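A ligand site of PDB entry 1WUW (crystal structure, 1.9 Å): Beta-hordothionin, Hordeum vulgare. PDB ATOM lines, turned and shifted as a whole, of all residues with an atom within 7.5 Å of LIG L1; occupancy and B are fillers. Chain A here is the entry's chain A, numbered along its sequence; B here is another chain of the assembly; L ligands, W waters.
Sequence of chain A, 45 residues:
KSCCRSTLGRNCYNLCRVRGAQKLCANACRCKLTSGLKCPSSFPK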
ATOM      1  N   CYS A   4       7.793  14.991  22.328  1.00  0.00           N
ATOM      2  CA  CYS A   4       7.061  13.961  21.615  1.00  0.00           C
ATOM      3  C   CYS A   4       6.113  14.575  20.583  1.00  0.00           C
ATOM      4  O   CYS A   4       5.798  15.757  20.597  1.00  0.00           O
ATOM      5  CB  CYS A   4       6.298  13.073  22.623  1.00  0.00           C
ATOM      6  SG  CYS A   4       7.485  12.115  23.611  1.00  0.00           S
ATOM      7  N   ARG A   5       5.636  13.782  19.639  1.00  0.00           N
ATOM      8  CA  ARG A   5       4.902  14.336  18.510  1.00  0.00           C
ATOM      9  C   ARG A   5       3.434  14.537  18.824  1.00  0.00           C
ATOM     10  O   ARG A   5       2.781  15.319  18.160  1.00  0.00           O
ATOM     11  CB  ARG A   5       4.981  13.388  17.312  1.00  0.00           C
ATOM     12  CG  ARG A   5       6.389  13.231  16.763  1.00  0.00           C
ATOM     13  CD  ARG A   5       6.428  12.035  15.801  1.00  0.00           C
ATOM     14  NE  ARG A   5       7.829  11.610  15.646  1.00  0.00           N
ATOM     15  CZ  ARG A   5       8.514  11.702  14.511  1.00  0.00           C
ATOM     16  NH1 ARG A   5       7.896  12.192  13.440  1.00  0.00           N
ATOM     17  NH2 ARG A   5       9.772  11.303  14.447  1.00  0.00           N
ATOM     18  N   SER A   6       2.981  13.766  19.810  1.00  0.00           N
ATOM     19  CA  SER A   6       1.551  13.707  20.065  1.00  0.00           C
ATOM     20  C   SER A   6       1.300  13.274  21.500  1.00  0.00           C
ATOM     21  O   SER A   6       2.220  12.897  22.214  1.00  0.00           O
ATOM     22  CB  SER A   6       0.871  12.720  19.117  1.00  0.00           C
ATOM     23  OG  SER A   6       1.366  11.407  19.372  1.00  0.00           O
ATOM     24  N   THR A   7       0.033  13.323  21.918  1.00  0.00           N
ATOM     25  CA  THR A   7      -0.313  12.889  23.275  1.00  0.00           C
ATOM     26  C   THR A   7      -0.066  11.389  23.408  1.00  0.00           C
ATOM     27  O   THR A   7       0.364  10.913  24.442  1.00  0.00           O
ATOM     28  CB  THR A   7      -1.798  13.250  23.544  1.00  0.00           C
ATOM     29  OG1 THR A   7      -1.823  14.675  23.740  1.00  0.00           O
ATOM     30  CG2 THR A   7      -2.329  12.603  24.800  1.00  0.00           C
ATOM     31  N   LEU A   8      -0.342  10.660  22.327  1.00  0.00           N
ATOM     32  CA  LEU A   8      -0.150   9.213  22.341  1.00  0.00           C
ATOM     33  C   LEU A   8       1.338   8.881  22.475  1.00  0.00           C
ATOM     34  O   LEU A   8       1.699   7.894  23.108  1.00  0.00           O
ATOM     35  CB  LEU A   8      -0.705   8.573  21.072  1.00  0.00           C
ATOM     36  CG  LEU A   8      -2.240   8.474  21.009  1.00  0.00           C
ATOM     37  CD1 LEU A   8      -2.674   7.987  19.635  1.00  0.00           C
ATOM     38  CD2 LEU A   8      -2.742   7.557  22.113  1.00  0.00           C
ATOM     39  N   GLY A   9       2.175   9.717  21.863  1.00  0.00           N
ATOM     40  CA  GLY A   9       3.619   9.563  21.938  1.00  0.00           C
ATOM     41  C   GLY A   9       4.133   9.866  23.323  1.00  0.00           C
ATOM     42  O   GLY A   9       5.031   9.205  23.833  1.00  0.00           O
ATOM     43  N   ARG A  10       3.589  10.889  23.972  1.00  0.00           N
ATOM     44  CA  ARG A  10       3.950  11.213  25.346  1.00  0.00           C
ATOM     45  C   ARG A  10       3.579  10.075  26.288  1.00  0.00           C
ATOM     46  O   ARG A  10       4.358   9.707  27.183  1.00  0.00           O
ATOM     47  CB  ARG A  10       3.250  12.538  25.730  1.00  0.00           C
ATOM     48  CG  ARG A  10       3.429  12.910  27.184  1.00  0.00           C
ATOM     49  CD  ARG A  10       4.886  12.972  27.595  1.00  0.00           C
ATOM     50  NE  ARG A  10       5.669  13.951  26.830  1.00  0.00           N
ATOM     51  CZ  ARG A  10       6.990  13.992  26.977  1.00  0.00           C
ATOM     52  NH1 ARG A  10       7.563  13.137  27.806  1.00  0.00           N
ATOM     53  NH2 ARG A  10       7.741  14.847  26.308  1.00  0.00           N
ATOM     54  N   ASN A  11       2.367   9.536  26.090  1.00  0.00           N
ATOM     55  CA  ASN A  11       1.919   8.398  26.921  1.00  0.00           C
ATOM     56  C   ASN A  11       2.868   7.216  26.749  1.00  0.00           C
ATOM     57  O   ASN A  11       3.336   6.562  27.709  1.00  0.00           O
ATOM     58  CB  ASN A  11       0.496   7.968  26.544  1.00  0.00           C
ATOM     59  CG  ASN A  11      -0.018   6.864  27.458  1.00  0.00           C
ATOM     60  OD1 ASN A  11      -0.061   7.068  28.677  1.00  0.00           O
ATOM     61  ND2 ASN A  11      -0.361   5.722  26.878  1.00  0.00           N
ATOM     62  N   CYS A  12       3.178   6.934  25.481  1.00  0.00           N
ATOM     63  CA  CYS A  12       4.117   5.859  25.127  1.00  0.00           C
ATOM     64  C   CYS A  12       5.399   6.043  25.907  1.00  0.00           C
ATOM     65  O   CYS A  12       5.940   5.159  26.579  1.00  0.00           O
ATOM     66  CB  CYS A  12       4.379   5.903  23.615  1.00  0.00           C
ATOM     67  SG  CYS A  12       5.507   4.647  22.952  1.00  0.00           S
ATOM     68  N   TYR A  13       5.964   7.239  25.780  1.00  0.00           N
ATOM     69  CA  TYR A  13       7.259   7.529  26.380  1.00  0.00           C
ATOM     70  C   TYR A  13       7.229   7.386  27.897  1.00  0.00           C
ATOM     71  O   TYR A  13       8.133   6.772  28.497  1.00  0.00           O
ATOM     72  CB  TYR A  13       7.707   8.938  25.989  1.00  0.00           C
ATOM     73  CG  TYR A  13       9.086   9.294  26.520  1.00  0.00           C
ATOM     74  CD1 TYR A  13       9.256  10.054  27.672  1.00  0.00           C
ATOM     75  CD2 TYR A  13      10.237   8.868  25.855  1.00  0.00           C
ATOM     76  CE1 TYR A  13      10.519  10.368  28.160  1.00  0.00           C
ATOM     77  CE2 TYR A  13      11.490   9.182  26.333  1.00  0.00           C
ATOM     78  CZ  TYR A  13      11.633   9.926  27.488  1.00  0.00           C
ATOM     79  OH  TYR A  13      12.904  10.216  27.932  1.00  0.00           O
ATOM     80  N   ALA A  28      11.541   4.230  20.516  1.00  0.00           N
ATOM     81  CA  ALA A  28      10.315   3.435  20.451  1.00  0.00           C
ATOM     82  C   ALA A  28       9.084   4.275  20.194  1.00  0.00           C
ATOM     83  O   ALA A  28       8.221   3.859  19.444  1.00  0.00           O
ATOM     84  CB  ALA A  28      10.096   2.678  21.774  1.00  0.00           C
ATOM     85  N   CYS A  29       9.042   5.437  20.863  1.00  0.00           N
ATOM     86  CA  CYS A  29       7.817   6.234  20.830  1.00  0.00           C
ATOM     87  C   CYS A  29       7.897   7.395  19.845  1.00  0.00           C
ATOM     88  O   CYS A  29       6.999   8.227  19.827  1.00  0.00           O
ATOM     89  CB  CYS A  29       7.545   6.765  22.240  1.00  0.00           C
ATOM     90  SG  CYS A  29       7.334   5.372  23.380  1.00  0.00           S
ATOM     91  N   ARG A  30       8.965   7.434  19.071  1.00  0.00           N
ATOM     92  CA  ARG A  30       9.218   8.460  18.076  1.00  0.00           C
ATOM     93  C   ARG A  30       9.214   9.865  18.695  1.00  0.00           C
ATOM     94  O   ARG A  30       8.585  10.761  18.152  1.00  0.00           O
ATOM     95  CB  ARG A  30       8.185   8.407  16.946  1.00  0.00           C
ATOM     96  CG  ARG A  30       8.060   7.063  16.235  1.00  0.00           C
ATOM     97  CD  ARG A  30       6.832   7.067  15.333  1.00  0.00           C
ATOM     98  NE  ARG A  30       7.077   7.712  14.066  1.00  0.00           N
ATOM     99  CZ  ARG A  30       6.338   8.481  13.307  1.00  0.00           C
ATOM    100  NH1 ARG A  30       5.086   8.849  13.568  1.00  0.00           N
ATOM    101  NH2 ARG A  30       6.905   8.912  12.181  1.00  0.00           N
ATOM    102  N   CYS A  31       9.899  10.034  19.805  1.00  0.00           N
ATOM    103  CA  CYS A  31      10.086  11.301  20.490  1.00  0.00           C
ATOM    104  C   CYS A  31      11.513  11.728  20.212  1.00  0.00           C
ATOM    105  O   CYS A  31      12.215  10.868  19.685  1.00  0.00           O
ATOM    106  CB  CYS A  31       9.860  11.176  22.006  1.00  0.00           C
ATOM    107  SG  CYS A  31       8.146  10.663  22.345  1.00  0.00           S
ATOM    108  N   PHE A  43       7.679  18.850  17.814  1.00  0.00           N
ATOM    109  CA  PHE A  43       7.686  17.849  18.897  1.00  0.00           C
ATOM    110  C   PHE A  43       7.284  18.519  20.208  1.00  0.00           C
ATOM    111  O   PHE A  43       8.026  18.647  21.187  1.00  0.00           O
ATOM    112  CB  PHE A  43       9.037  17.164  18.995  1.00  0.00           C
ATOM    113  CG  PHE A  43       9.448  16.324  17.791  1.00  0.00           C
ATOM    114  CD1 PHE A  43       9.854  16.917  16.609  1.00  0.00           C
ATOM    115  CD2 PHE A  43       9.440  14.950  17.863  1.00  0.00           C
ATOM    116  CE1 PHE A  43      10.235  16.135  15.533  1.00  0.00           C
ATOM    117  CE2 PHE A  43       9.807  14.147  16.789  1.00  0.00           C
ATOM    118  CZ  PHE A  43      10.209  14.749  15.611  1.00  0.00           C
ATOM    119  N   ARG B   5      -0.785  -2.719  15.462  1.00  0.00           N
ATOM    120  CA  ARG B   5      -1.550  -2.137  14.369  1.00  0.00           C
ATOM    121  C   ARG B   5      -0.758  -1.944  13.094  1.00  0.00           C
ATOM    122  O   ARG B   5      -1.290  -2.033  11.989  1.00  0.00           O
ATOM    123  CB  ARG B   5      -2.111  -0.743  14.742  1.00  0.00           C
ATOM    124  CG  ARG B   5      -3.213  -0.776  15.774  1.00  0.00           C
ATOM    125  CD  ARG B   5      -3.405   0.536  16.527  1.00  0.00           C
ATOM    126  NE  ARG B   5      -4.067   0.342  17.823  1.00  0.00           N
ATOM    127  CZ  ARG B   5      -5.329   0.649  18.098  1.00  0.00           C
ATOM    128  NH1 ARG B   5      -6.128   1.197  17.190  1.00  0.00           N
ATOM    129  NH2 ARG B   5      -5.804   0.419  19.321  1.00  0.00           N
ATOM    130  N   LEU B   8       5.109   0.539  12.783  1.00  0.00           N
ATOM    131  CA  LEU B   8       5.565   1.505  13.778  1.00  0.00           C
ATOM    132  C   LEU B   8       5.300   0.967  15.185  1.00  0.00           C
ATOM    133  O   LEU B   8       6.130   1.113  16.072  1.00  0.00           O
ATOM    134  CB  LEU B   8       4.844   2.845  13.648  1.00  0.00           C
ATOM    135  CG  LEU B   8       4.896   3.563  12.295  1.00  0.00           C
ATOM    136  CD1 LEU B   8       4.306   4.960  12.425  1.00  0.00           C
ATOM    137  CD2 LEU B   8       6.323   3.621  11.784  1.00  0.00           C
ATOM    138  N   GLY B   9       4.103   0.394  15.359  1.00  0.00           N
ATOM    139  CA  GLY B   9       3.712  -0.173  16.630  1.00  0.00           C
ATOM    140  C   GLY B   9       4.525  -1.401  16.991  1.00  0.00           C
ATOM    141  O   GLY B   9       4.913  -1.610  18.142  1.00  0.00           O
ATOM    142  N   CYS B  12       7.917  -0.177  18.040  1.00  0.00           N
ATOM    143  CA  CYS B  12       7.752   0.388  19.399  1.00  0.00           C
ATOM    144  C   CYS B  12       7.793  -0.739  20.422  1.00  0.00           C
ATOM    145  O   CYS B  12       8.512  -0.693  21.417  1.00  0.00           O
ATOM    146  CB  CYS B  12       6.425   1.146  19.459  1.00  0.00           C
ATOM    147  SG  CYS B  12       5.985   1.870  21.050  1.00  0.00           S
ATOM    148  N   ALA B  26       2.566  -3.233  25.549  1.00  0.00           N
ATOM    149  CA  ALA B  26       1.383  -3.309  24.709  1.00  0.00           C
ATOM    150  C   ALA B  26       0.551  -2.030  24.861  1.00  0.00           C
ATOM    151  O   ALA B  26       0.092  -1.396  23.902  1.00  0.00           O
ATOM    152  CB  ALA B  26       0.547  -4.526  25.060  1.00  0.00           C
ATOM    153  N   ASN B  27       0.358  -1.601  26.110  1.00  0.00           N
ATOM    154  CA  ASN B  27      -0.362  -0.348  26.316  1.00  0.00           C
ATOM    155  C   ASN B  27       0.424   0.842  25.785  1.00  0.00           C
ATOM    156  O   ASN B  27      -0.165   1.764  25.210  1.00  0.00           O
ATOM    157  CB  ASN B  27      -0.640  -0.092  27.804  1.00  0.00           C
ATOM    158  CG  ASN B  27      -1.781  -0.913  28.348  1.00  0.00           C
ATOM    159  OD1 ASN B  27      -2.118  -1.945  27.776  1.00  0.00           O
ATOM    160  ND2 ASN B  27      -2.333  -0.412  29.456  1.00  0.00           N
ATOM    161  N   ALA B  28       1.732   0.923  25.962  1.00  0.00           N
ATOM    162  CA  ALA B  28       2.446   2.076  25.426  1.00  0.00           C
ATOM    163  C   ALA B  28       2.368   2.207  23.914  1.00  0.00           C
ATOM    164  O   ALA B  28       2.308   3.289  23.346  1.00  0.00           O
ATOM    165  CB  ALA B  28       3.928   1.935  25.772  1.00  0.00           C
ATOM    166  N   CYS B  29       2.405   1.049  23.257  1.00  0.00           N
ATOM    167  CA  CYS B  29       2.559   1.010  21.796  1.00  0.00           C
ATOM    168  C   CYS B  29       1.273   0.690  21.061  1.00  0.00           C
ATOM    169  O   CYS B  29       1.320   0.449  19.847  1.00  0.00           O
ATOM    170  CB  CYS B  29       3.633  -0.041  21.442  1.00  0.00           C
ATOM    171  SG  CYS B  29       5.233   0.358  22.158  1.00  0.00           S
ATOM    172  N   ARG B  30       0.137   0.675  21.735  1.00  0.00           N
ATOM    173  CA  ARG B  30      -1.175   0.334  21.223  1.00  0.00           C
ATOM    174  C   ARG B  30      -1.229  -1.019  20.507  1.00  0.00           C
ATOM    175  O   ARG B  30      -1.894  -1.146  19.484  1.00  0.00           O
ATOM    176  CB  ARG B  30      -1.663   1.386  20.210  1.00  0.00           C
ATOM    177  CG  ARG B  30      -1.722   2.791  20.818  1.00  0.00           C
ATOM    178  CD  ARG B  30      -1.996   3.818  19.738  1.00  0.00           C
ATOM    179  NE  ARG B  30      -3.356   3.755  19.236  1.00  0.00           N
ATOM    180  CZ  ARG B  30      -3.747   4.174  18.031  1.00  0.00           C
ATOM    181  NH1 ARG B  30      -2.900   4.686  17.152  1.00  0.00           N
ATOM    182  NH2 ARG B  30      -5.020   4.068  17.687  1.00  0.00           N
ATOM    183  N   CYS B  31      -0.551  -2.006  21.061  1.00  0.00           N
ATOM    184  CA  CYS B  31      -0.706  -3.386  20.622  1.00  0.00           C
ATOM    185  C   CYS B  31      -1.669  -4.115  21.562  1.00  0.00           C
ATOM    186  O   CYS B  31      -1.971  -3.607  22.629  1.00  0.00           O
ATOM    187  CB  CYS B  31       0.645  -4.083  20.591  1.00  0.00           C
ATOM    188  SG  CYS B  31       1.873  -3.167  19.638  1.00  0.00           S
HETATM  189  S1  LIG L   1       3.321   9.360  17.005  1.00  0.00           S
HETATM  190  O1  LIG L   1       2.850   9.248  15.655  1.00  0.00           O
HETATM  191  O2  LIG L   1       2.815  10.711  17.578  1.00  0.00           O
HETATM  192  O3  LIG L   1       4.856   9.378  17.028  1.00  0.00           O
HETATM  193  C1  LIG L   1       2.690   8.072  17.964  1.00  0.00           C
HETATM  194  C2  LIG L   1       3.438   7.613  19.039  1.00  0.00           C
HETATM  195  C3  LIG L   1       2.905   6.591  19.815  1.00  0.00           C
HETATM  196  C4  LIG L   1       1.661   6.047  19.515  1.00  0.00           C
HETATM  197  C5  LIG L   1       0.909   6.543  18.437  1.00  0.00           C
HETATM  198  C6  LIG L   1       1.455   7.541  17.649  1.00  0.00           C
HETATM  199  C7  LIG L   1       1.137   4.905  20.345  1.00  0.00           C
HETATM  200  S1  LG2 L   2       0.037   2.662  15.790  1.00  0.00           S
HETATM  201  O1  LG2 L   2       0.400   1.707  14.797  1.00  0.00           O
HETATM  202  O2  LG2 L   2      -0.728   1.946  16.925  1.00  0.00           O
HETATM  203  O3  LG2 L   2      -0.846   3.763  15.180  1.00  0.00           O
HETATM  204  C1  LG2 L   2       1.487   3.358  16.439  1.00  0.00           C
HETATM  205  C2  LG2 L   2       2.074   4.410  15.766  1.00  0.00           C
HETATM  206  C3  LG2 L   2       3.279   4.942  16.226  1.00  0.00           C
HETATM  207  C4  LG2 L   2       3.888   4.372  17.347  1.00  0.00           C
HETATM  208  C5  LG2 L   2       3.283   3.317  18.008  1.00  0.00           C
HETATM  209  C6  LG2 L   2       2.064   2.806  17.569  1.00  0.00           C
HETATM  210  C7  LG2 L   2       5.139   5.016  17.883  1.00  0.00           C
HETATM  211  O   HOH W   1       5.725  10.939  19.483  1.00  0.00           O
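The side-chain hydroxyl (OG) of Ser 6 lies within hydrogen-bond range of an oxygen (O2) of LIG L1 (2.4 Å).
An oxygen (O3) of LIG L1 is in salt-bridge range of the guanidinium group of Arg 5 of chain A.
NE of Arg 5 of chain B lies within salt-bridge range of O2 of LG2 L2.
An oxygen (O1) of LIG L1 lies within salt-bridge range of the guanidinium group of Arg 30 of chain A, at 3.1 Å.
NH1 of Arg 30 of chain B lies within salt-bridge range of O3 of LG2 L2 (3.0 Å).
Merely in contact with LIG L1: Arg 30 of chain B (3.4 Å), Gly 9 of chain A (3.5 Å), Ala 28 of chain B (3.6 Å), Leu 8 of chain A (3.7 Å) and Cys 29 of chain A (3.7 Å).
Eight residues have an atom within 4 Å of LIG L1: Arg 5 of chain A, Ser 6, Leu 8 of chain A, Gly 9 of chain A, Cys 29 of chain A, Arg 30 of chain A, Ala 28 of chain B and Arg 30 of chain B.
The nearest printed residue that does not touch LIG L1 is Cys 12 of chain A (4.1 Å).
The backbone carbonyl oxygen (O) of Arg 30 of chain B is in hydrogen-bond range of the guanidinium group (NE) of Arg 5 of chain B, 3.1 Å away.
The backbone carbonyl oxygen of Arg 30 of chain A sits at hydrogen-bond distance from the guanidinium group of Arg 5 of chain A.
N of Gly 9 of chain A lies within hydrogen-bond range of OG of Ser 6 (3.1 Å).
The side-chain sulfur (SG) of Cys 4 forms a disulfide with the side-chain sulfur (SG) of Cys 31 of chain A, at 2.0 Å.
N of Leu 8 of chain A sits close to OG of Ser 6, 3.5 Å away.
SG of Cys 12 of chain A forms a disulfide with SG of Cys 29 of chain A (2.0 Å).
SG of Cys 29 of chain B is disulfide-bonded to SG of Cys 12 of chain B, at 2.0 Å.
N of Tyr 13 sits at hydrogen-bond distance from SG of Cys 29 of chain A, 3.3 Å away.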
